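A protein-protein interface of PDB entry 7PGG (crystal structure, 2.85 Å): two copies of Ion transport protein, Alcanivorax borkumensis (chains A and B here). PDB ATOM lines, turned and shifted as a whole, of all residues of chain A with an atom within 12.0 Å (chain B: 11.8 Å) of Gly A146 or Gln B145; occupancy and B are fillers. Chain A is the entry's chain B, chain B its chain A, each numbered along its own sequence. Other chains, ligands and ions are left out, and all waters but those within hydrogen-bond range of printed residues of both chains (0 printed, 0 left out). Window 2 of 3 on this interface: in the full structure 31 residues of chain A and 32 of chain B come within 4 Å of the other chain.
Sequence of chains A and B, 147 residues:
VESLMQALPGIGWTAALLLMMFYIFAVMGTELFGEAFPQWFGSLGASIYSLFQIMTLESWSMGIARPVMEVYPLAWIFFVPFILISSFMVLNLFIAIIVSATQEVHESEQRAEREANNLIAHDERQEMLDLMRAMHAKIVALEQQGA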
ATOM      1  N   ALA A 137      -7.478  -0.445 -16.840  1.00  0.00           N
ATOM      2  CA  ALA A 137      -7.903   0.875 -17.292  1.00  0.00           C
ATOM      3  C   ALA A 137      -9.095   1.377 -16.488  1.00  0.00           C
ATOM      4  O   ALA A 137      -9.158   2.557 -16.127  1.00  0.00           O
ATOM      5  CB  ALA A 137      -8.239   0.834 -18.782  1.00  0.00           C
ATOM      6  N   LYS A 138     -10.049   0.493 -16.189  1.00  0.00           N
ATOM      7  CA  LYS A 138     -11.215   0.919 -15.429  1.00  0.00           C
ATOM      8  C   LYS A 138     -10.860   1.260 -13.990  1.00  0.00           C
ATOM      9  O   LYS A 138     -11.462   2.171 -13.409  1.00  0.00           O
ATOM     10  CB  LYS A 138     -12.312  -0.135 -15.502  1.00  0.00           C
ATOM     11  CG  LYS A 138     -12.809  -0.215 -16.934  1.00  0.00           C
ATOM     12  CD  LYS A 138     -14.142  -0.804 -17.080  1.00  0.00           C
ATOM     13  CE  LYS A 138     -14.663  -0.908 -18.509  1.00  0.00           C
ATOM     14  NZ  LYS A 138     -15.236   0.325 -19.108  1.00  0.00           N
ATOM     15  N   ILE A 139      -9.890   0.552 -13.408  1.00  0.00           N
ATOM     16  CA  ILE A 139      -9.380   0.902 -12.081  1.00  0.00           C
ATOM     17  C   ILE A 139      -8.840   2.327 -12.091  1.00  0.00           C
ATOM     18  O   ILE A 139      -9.164   3.149 -11.224  1.00  0.00           O
ATOM     19  CB  ILE A 139      -8.263  -0.072 -11.677  1.00  0.00           C
ATOM     20  CG1 ILE A 139      -8.662  -1.553 -11.708  1.00  0.00           C
ATOM     21  CG2 ILE A 139      -7.780   0.285 -10.278  1.00  0.00           C
ATOM     22  CD1 ILE A 139      -9.215  -2.144 -10.545  1.00  0.00           C
ATOM     23  N   VAL A 140      -7.978   2.623 -13.069  1.00  0.00           N
ATOM     24  CA  VAL A 140      -7.350   3.938 -13.161  1.00  0.00           C
ATOM     25  C   VAL A 140      -8.402   5.014 -13.397  1.00  0.00           C
ATOM     26  O   VAL A 140      -8.283   6.138 -12.896  1.00  0.00           O
ATOM     27  CB  VAL A 140      -6.274   3.928 -14.267  1.00  0.00           C
ATOM     28  CG1 VAL A 140      -5.656   5.303 -14.443  1.00  0.00           C
ATOM     29  CG2 VAL A 140      -5.206   2.905 -13.945  1.00  0.00           C
ATOM     30  N   ALA A 141      -9.449   4.685 -14.158  1.00  0.00           N
ATOM     31  CA  ALA A 141     -10.551   5.624 -14.352  1.00  0.00           C
ATOM     32  C   ALA A 141     -11.235   5.939 -13.029  1.00  0.00           C
ATOM     33  O   ALA A 141     -11.446   7.114 -12.694  1.00  0.00           O
ATOM     34  CB  ALA A 141     -11.561   5.065 -15.354  1.00  0.00           C
ATOM     35  N   LEU A 142     -11.579   4.902 -12.245  1.00  0.00           N
ATOM     36  CA  LEU A 142     -12.275   5.186 -10.997  1.00  0.00           C
ATOM     37  C   LEU A 142     -11.337   5.876 -10.016  1.00  0.00           C
ATOM     38  O   LEU A 142     -11.797   6.537  -9.078  1.00  0.00           O
ATOM     39  CB  LEU A 142     -12.788   3.961 -10.243  1.00  0.00           C
ATOM     40  CG  LEU A 142     -13.417   2.581 -10.073  1.00  0.00           C
ATOM     41  CD1 LEU A 142     -14.023   2.570  -8.652  1.00  0.00           C
ATOM     42  CD2 LEU A 142     -14.352   2.035 -11.101  1.00  0.00           C
ATOM     43  N   GLU A 143     -10.027   5.672 -10.173  1.00  0.00           N
ATOM     44  CA  GLU A 143      -9.059   6.309  -9.283  1.00  0.00           C
ATOM     45  C   GLU A 143      -8.962   7.807  -9.556  1.00  0.00           C
ATOM     46  O   GLU A 143      -8.795   8.608  -8.631  1.00  0.00           O
ATOM     47  CB  GLU A 143      -7.692   5.646  -9.442  1.00  0.00           C
ATOM     48  CG  GLU A 143      -6.628   6.175  -8.504  1.00  0.00           C
ATOM     49  CD  GLU A 143      -5.319   5.441  -8.661  1.00  0.00           C
ATOM     50  OE1 GLU A 143      -5.255   4.541  -9.521  1.00  0.00           O
ATOM     51  OE2 GLU A 143      -4.360   5.760  -7.926  1.00  0.00           O
ATOM     52  N   GLN A 144      -9.042   8.191 -10.830  1.00  0.00           N
ATOM     53  CA  GLN A 144      -9.175   9.591 -11.224  1.00  0.00           C
ATOM     54  C   GLN A 144     -10.413  10.254 -10.662  1.00  0.00           C
ATOM     55  O   GLN A 144     -10.365  11.433 -10.291  1.00  0.00           O
ATOM     56  CB  GLN A 144      -9.069   9.624 -12.747  1.00  0.00           C
ATOM     57  CG  GLN A 144      -7.664   9.894 -12.981  1.00  0.00           C
ATOM     58  CD  GLN A 144      -6.798   9.263 -14.009  1.00  0.00           C
ATOM     59  OE1 GLN A 144      -6.986   8.151 -14.492  1.00  0.00           O
ATOM     60  NE2 GLN A 144      -5.766  10.012 -14.334  1.00  0.00           N
ATOM     61  N   GLN A 145     -11.506   9.511 -10.542  1.00  0.00           N
ATOM     62  CA  GLN A 145     -12.720  10.075  -9.976  1.00  0.00           C
ATOM     63  C   GLN A 145     -12.561  10.438  -8.505  1.00  0.00           C
ATOM     64  O   GLN A 145     -13.371  11.213  -7.984  1.00  0.00           O
ATOM     65  CB  GLN A 145     -13.878   9.091 -10.149  1.00  0.00           C
ATOM     66  CG  GLN A 145     -14.279   8.853 -11.594  1.00  0.00           C
ATOM     67  CD  GLN A 145     -15.417   7.856 -11.723  1.00  0.00           C
ATOM     68  OE1 GLN A 145     -15.878   7.287 -10.730  1.00  0.00           O
ATOM     69  NE2 GLN A 145     -15.871   7.635 -12.948  1.00  0.00           N
ATOM     70  N   GLY A 146     -11.548   9.899  -7.826  1.00  0.00           N
ATOM     71  CA  GLY A 146     -11.322  10.208  -6.427  1.00  0.00           C
ATOM     72  C   GLY A 146     -10.357  11.359  -6.228  1.00  0.00           C
ATOM     73  O   GLY A 146     -10.651  12.286  -5.468  1.00  0.00           O
ATOM     74  N   ALA A 147      -9.217  11.299  -6.922  1.00  0.00           N
ATOM     75  CA  ALA A 147      -8.146  12.314  -6.927  1.00  0.00           C
ATOM     76  C   ALA A 147      -8.271  13.436  -5.896  1.00  0.00           C
ATOM     77  O   ALA A 147      -8.920  14.453  -6.147  1.00  0.00           O
ATOM     78  CB  ALA A 147      -8.036  12.924  -8.321  1.00  0.00           C
ATOM     79  N   HIS B 136      -3.327  -4.379  -8.326  1.00  0.00           N
ATOM     80  CA  HIS B 136      -3.653  -4.561  -6.913  1.00  0.00           C
ATOM     81  C   HIS B 136      -3.210  -3.379  -6.069  1.00  0.00           C
ATOM     82  O   HIS B 136      -3.907  -3.006  -5.119  1.00  0.00           O
ATOM     83  CB  HIS B 136      -3.111  -5.922  -6.449  1.00  0.00           C
ATOM     84  CG  HIS B 136      -3.144  -6.167  -4.971  1.00  0.00           C
ATOM     85  ND1 HIS B 136      -4.079  -5.601  -4.134  1.00  0.00           N
ATOM     86  CD2 HIS B 136      -2.622  -7.202  -4.271  1.00  0.00           C
ATOM     87  CE1 HIS B 136      -3.951  -6.107  -2.921  1.00  0.00           C
ATOM     88  NE2 HIS B 136      -3.098  -7.111  -2.985  1.00  0.00           N
ATOM     89  N   ALA B 137      -2.110  -2.731  -6.440  1.00  0.00           N
ATOM     90  CA  ALA B 137      -1.706  -1.516  -5.740  1.00  0.00           C
ATOM     91  C   ALA B 137      -2.728  -0.397  -5.925  1.00  0.00           C
ATOM     92  O   ALA B 137      -3.045   0.329  -4.975  1.00  0.00           O
ATOM     93  CB  ALA B 137      -0.330  -1.072  -6.225  1.00  0.00           C
ATOM     94  N   LYS B 138      -3.236  -0.228  -7.149  1.00  0.00           N
ATOM     95  CA  LYS B 138      -4.231   0.808  -7.425  1.00  0.00           C
ATOM     96  C   LYS B 138      -5.511   0.563  -6.636  1.00  0.00           C
ATOM     97  O   LYS B 138      -6.169   1.512  -6.193  1.00  0.00           O
ATOM     98  CB  LYS B 138      -4.540   0.825  -8.922  1.00  0.00           C
ATOM     99  CG  LYS B 138      -3.402   1.115  -9.902  1.00  0.00           C
ATOM    100  CD  LYS B 138      -3.106   2.516 -10.188  1.00  0.00           C
ATOM    101  CE  LYS B 138      -2.001   2.693 -11.203  1.00  0.00           C
ATOM    102  NZ  LYS B 138      -1.587   4.108 -11.097  1.00  0.00           N
ATOM    103  N   ILE B 139      -5.893  -0.707  -6.467  1.00  0.00           N
ATOM    104  CA  ILE B 139      -7.091  -1.016  -5.691  1.00  0.00           C
ATOM    105  C   ILE B 139      -6.903  -0.610  -4.241  1.00  0.00           C
ATOM    106  O   ILE B 139      -7.777   0.018  -3.631  1.00  0.00           O
ATOM    107  CB  ILE B 139      -7.468  -2.502  -5.824  1.00  0.00           C
ATOM    108  CG1 ILE B 139      -7.807  -2.718  -7.284  1.00  0.00           C
ATOM    109  CG2 ILE B 139      -8.621  -2.877  -4.909  1.00  0.00           C
ATOM    110  CD1 ILE B 139      -8.475  -3.894  -7.630  1.00  0.00           C
ATOM    111  N   VAL B 140      -5.750  -0.955  -3.674  1.00  0.00           N
ATOM    112  CA  VAL B 140      -5.460  -0.606  -2.291  1.00  0.00           C
ATOM    113  C   VAL B 140      -5.403   0.906  -2.117  1.00  0.00           C
ATOM    114  O   VAL B 140      -5.806   1.436  -1.074  1.00  0.00           O
ATOM    115  CB  VAL B 140      -4.155  -1.303  -1.857  1.00  0.00           C
ATOM    116  CG1 VAL B 140      -3.770  -0.926  -0.457  1.00  0.00           C
ATOM    117  CG2 VAL B 140      -4.314  -2.810  -1.966  1.00  0.00           C
ATOM    118  N   ALA B 141      -4.921   1.626  -3.134  1.00  0.00           N
ATOM    119  CA  ALA B 141      -4.893   3.086  -3.072  1.00  0.00           C
ATOM    120  C   ALA B 141      -6.303   3.662  -2.999  1.00  0.00           C
ATOM    121  O   ALA B 141      -6.615   4.478  -2.125  1.00  0.00           O
ATOM    122  CB  ALA B 141      -4.150   3.645  -4.288  1.00  0.00           C
ATOM    123  N   LEU B 142      -7.161   3.254  -3.925  1.00  0.00           N
ATOM    124  CA  LEU B 142      -8.563   3.657  -3.931  1.00  0.00           C
ATOM    125  C   LEU B 142      -9.315   3.183  -2.693  1.00  0.00           C
ATOM    126  O   LEU B 142     -10.284   3.827  -2.273  1.00  0.00           O
ATOM    127  CB  LEU B 142      -9.111   3.163  -5.267  1.00  0.00           C
ATOM    128  CG  LEU B 142     -10.090   2.729  -6.343  1.00  0.00           C
ATOM    129  CD1 LEU B 142     -11.350   3.469  -6.530  1.00  0.00           C
ATOM    130  CD2 LEU B 142      -9.218   3.067  -7.577  1.00  0.00           C
ATOM    131  N   GLU B 143      -8.852   2.100  -2.066  1.00  0.00           N
ATOM    132  CA  GLU B 143      -9.466   1.650  -0.823  1.00  0.00           C
ATOM    133  C   GLU B 143      -9.084   2.553   0.344  1.00  0.00           C
ATOM    134  O   GLU B 143      -9.910   2.792   1.237  1.00  0.00           O
ATOM    135  CB  GLU B 143      -9.072   0.201  -0.543  1.00  0.00           C
ATOM    136  CG  GLU B 143      -9.740  -0.405   0.676  1.00  0.00           C
ATOM    137  CD  GLU B 143      -9.362  -1.857   0.865  1.00  0.00           C
ATOM    138  OE1 GLU B 143      -8.562  -2.365   0.052  1.00  0.00           O
ATOM    139  OE2 GLU B 143      -9.863  -2.487   1.820  1.00  0.00           O
ATOM    140  N   GLN B 144      -7.843   3.070   0.365  1.00  0.00           N
ATOM    141  CA  GLN B 144      -7.510   3.977   1.457  1.00  0.00           C
ATOM    142  C   GLN B 144      -8.288   5.283   1.306  1.00  0.00           C
ATOM    143  O   GLN B 144      -8.548   5.965   2.303  1.00  0.00           O
ATOM    144  CB  GLN B 144      -6.044   4.413   1.537  1.00  0.00           C
ATOM    145  CG  GLN B 144      -4.757   3.643   1.376  1.00  0.00           C
ATOM    146  CD  GLN B 144      -4.340   2.357   1.997  1.00  0.00           C
ATOM    147  OE1 GLN B 144      -4.145   1.443   1.228  1.00  0.00           O
ATOM    148  NE2 GLN B 144      -3.979   2.317   3.272  1.00  0.00           N
ATOM    149  N   GLN B 145      -8.624   5.675   0.068  1.00  0.00           N
ATOM    150  CA  GLN B 145      -9.390   6.901  -0.148  1.00  0.00           C
ATOM    151  C   GLN B 145     -10.778   6.826   0.471  1.00  0.00           C
ATOM    152  O   GLN B 145     -11.411   7.867   0.674  1.00  0.00           O
ATOM    153  CB  GLN B 145      -9.514   7.208  -1.645  1.00  0.00           C
ATOM    154  CG  GLN B 145      -8.205   7.568  -2.333  1.00  0.00           C
ATOM    155  CD  GLN B 145      -8.376   7.851  -3.816  1.00  0.00           C
ATOM    156  OE1 GLN B 145      -9.473   7.721  -4.366  1.00  0.00           O
ATOM    157  NE2 GLN B 145      -7.287   8.237  -4.473  1.00  0.00           N
ATOM    158  N   GLY B 146     -11.268   5.622   0.764  1.00  0.00           N
ATOM    159  CA  GLY B 146     -12.566   5.461   1.385  1.00  0.00           C
ATOM    160  C   GLY B 146     -12.487   5.405   2.896  1.00  0.00           C
ATOM    161  O   GLY B 146     -13.241   6.106   3.576  1.00  0.00           O
ATOM    162  N   ALA B 147     -11.574   4.576   3.412  1.00  0.00           N
ATOM    163  CA  ALA B 147     -11.288   4.378   4.845  1.00  0.00           C
ATOM    164  C   ALA B 147     -12.260   5.034   5.827  1.00  0.00           C
ATOM    165  O   ALA B 147     -12.098   6.201   6.189  1.00  0.00           O
ATOM    166  CB  ALA B 147      -9.871   4.855   5.149  1.00  0.00           C
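Ile B139 touches its own counterpart, Ile A139.
Leu A142 touches its own counterpart, Leu B142.
Glu A143 touches Lys B138, but with the chains exchanged Lys A138 does not touch Glu B143 (11.6 Å).
Glu A143 touches Leu B142, but with the chains exchanged Leu A142 does not touch Glu B143 (8.4 Å).
Positions printed for both chains: 137, 138, 139, 140, 141, 142, 143, 144, 145, 146 and 147.
Of the 7 pairs that touch across the chains among the printed residues, 2 have their exchanged pair printed and touching as well.
Printed residues of chain A that touch a printed residue of chain B: Ile A139, Leu A142, Glu A143 and Gly A146.
Hydrophobic or aromatic side chains of chain A within 4 Å of the printed part of chain B: Ile A139 and Leu A142.
Along chain B the printed residues that touch a printed residue of chain A span positions 138 to 145.
Among the printed residues, 7 pairs touch across the chains.
Of the printed residues of chain B, Ile A139 touches Lys B138, Ile B139 and Leu B142.
Printed residues of chain B within 4 Å of Leu A142: Leu B142.
Of chain B, only Lys B138 and Leu B142 come within 4 Å of Glu A143.
No residue of chain B comes within 4 Å of Gln A145.
Gly A146 touches just one residue of chain B: Gln B145.
Of the printed residues of chain A, Lys B138 touches Ile A139 (3.6 Å) and Glu A143 (3.0 Å).
Of the printed residues of chain A, Ile B139 touches Ile A139.
No residue of chain A comes within 4 Å of Ala B141.
No residue of chain A comes within 4 Å of Gln B144.
Of chain A, only Gly A146 comes within 4 Å of Gln B145.
No residue of chain A comes within 4 Å of Gly B146.
No residue of chain A comes within 4 Å of Ala B147.
The nearest residue of chain B that does not touch Gly A146 is Leu B142 (6.6 Å).
The nearest residue of chain A that does not touch Gln B145 is Ala A147 (4.4 Å).
Among the printed residues, pairs that only touch across the chains: Glu A143 with Lys B138 (3.0 Å), Ile A139 with Ile B139 (3.5 Å), Leu A142 with Leu B142 (3.5 Å), Glu A143 with Leu B142 (3.5 Å), Ile A139 with Lys B138 (3.6 Å), Ile A139 with Leu B142 (3.6 Å) and Gly A146 with Gln B145 (3.7 Å).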
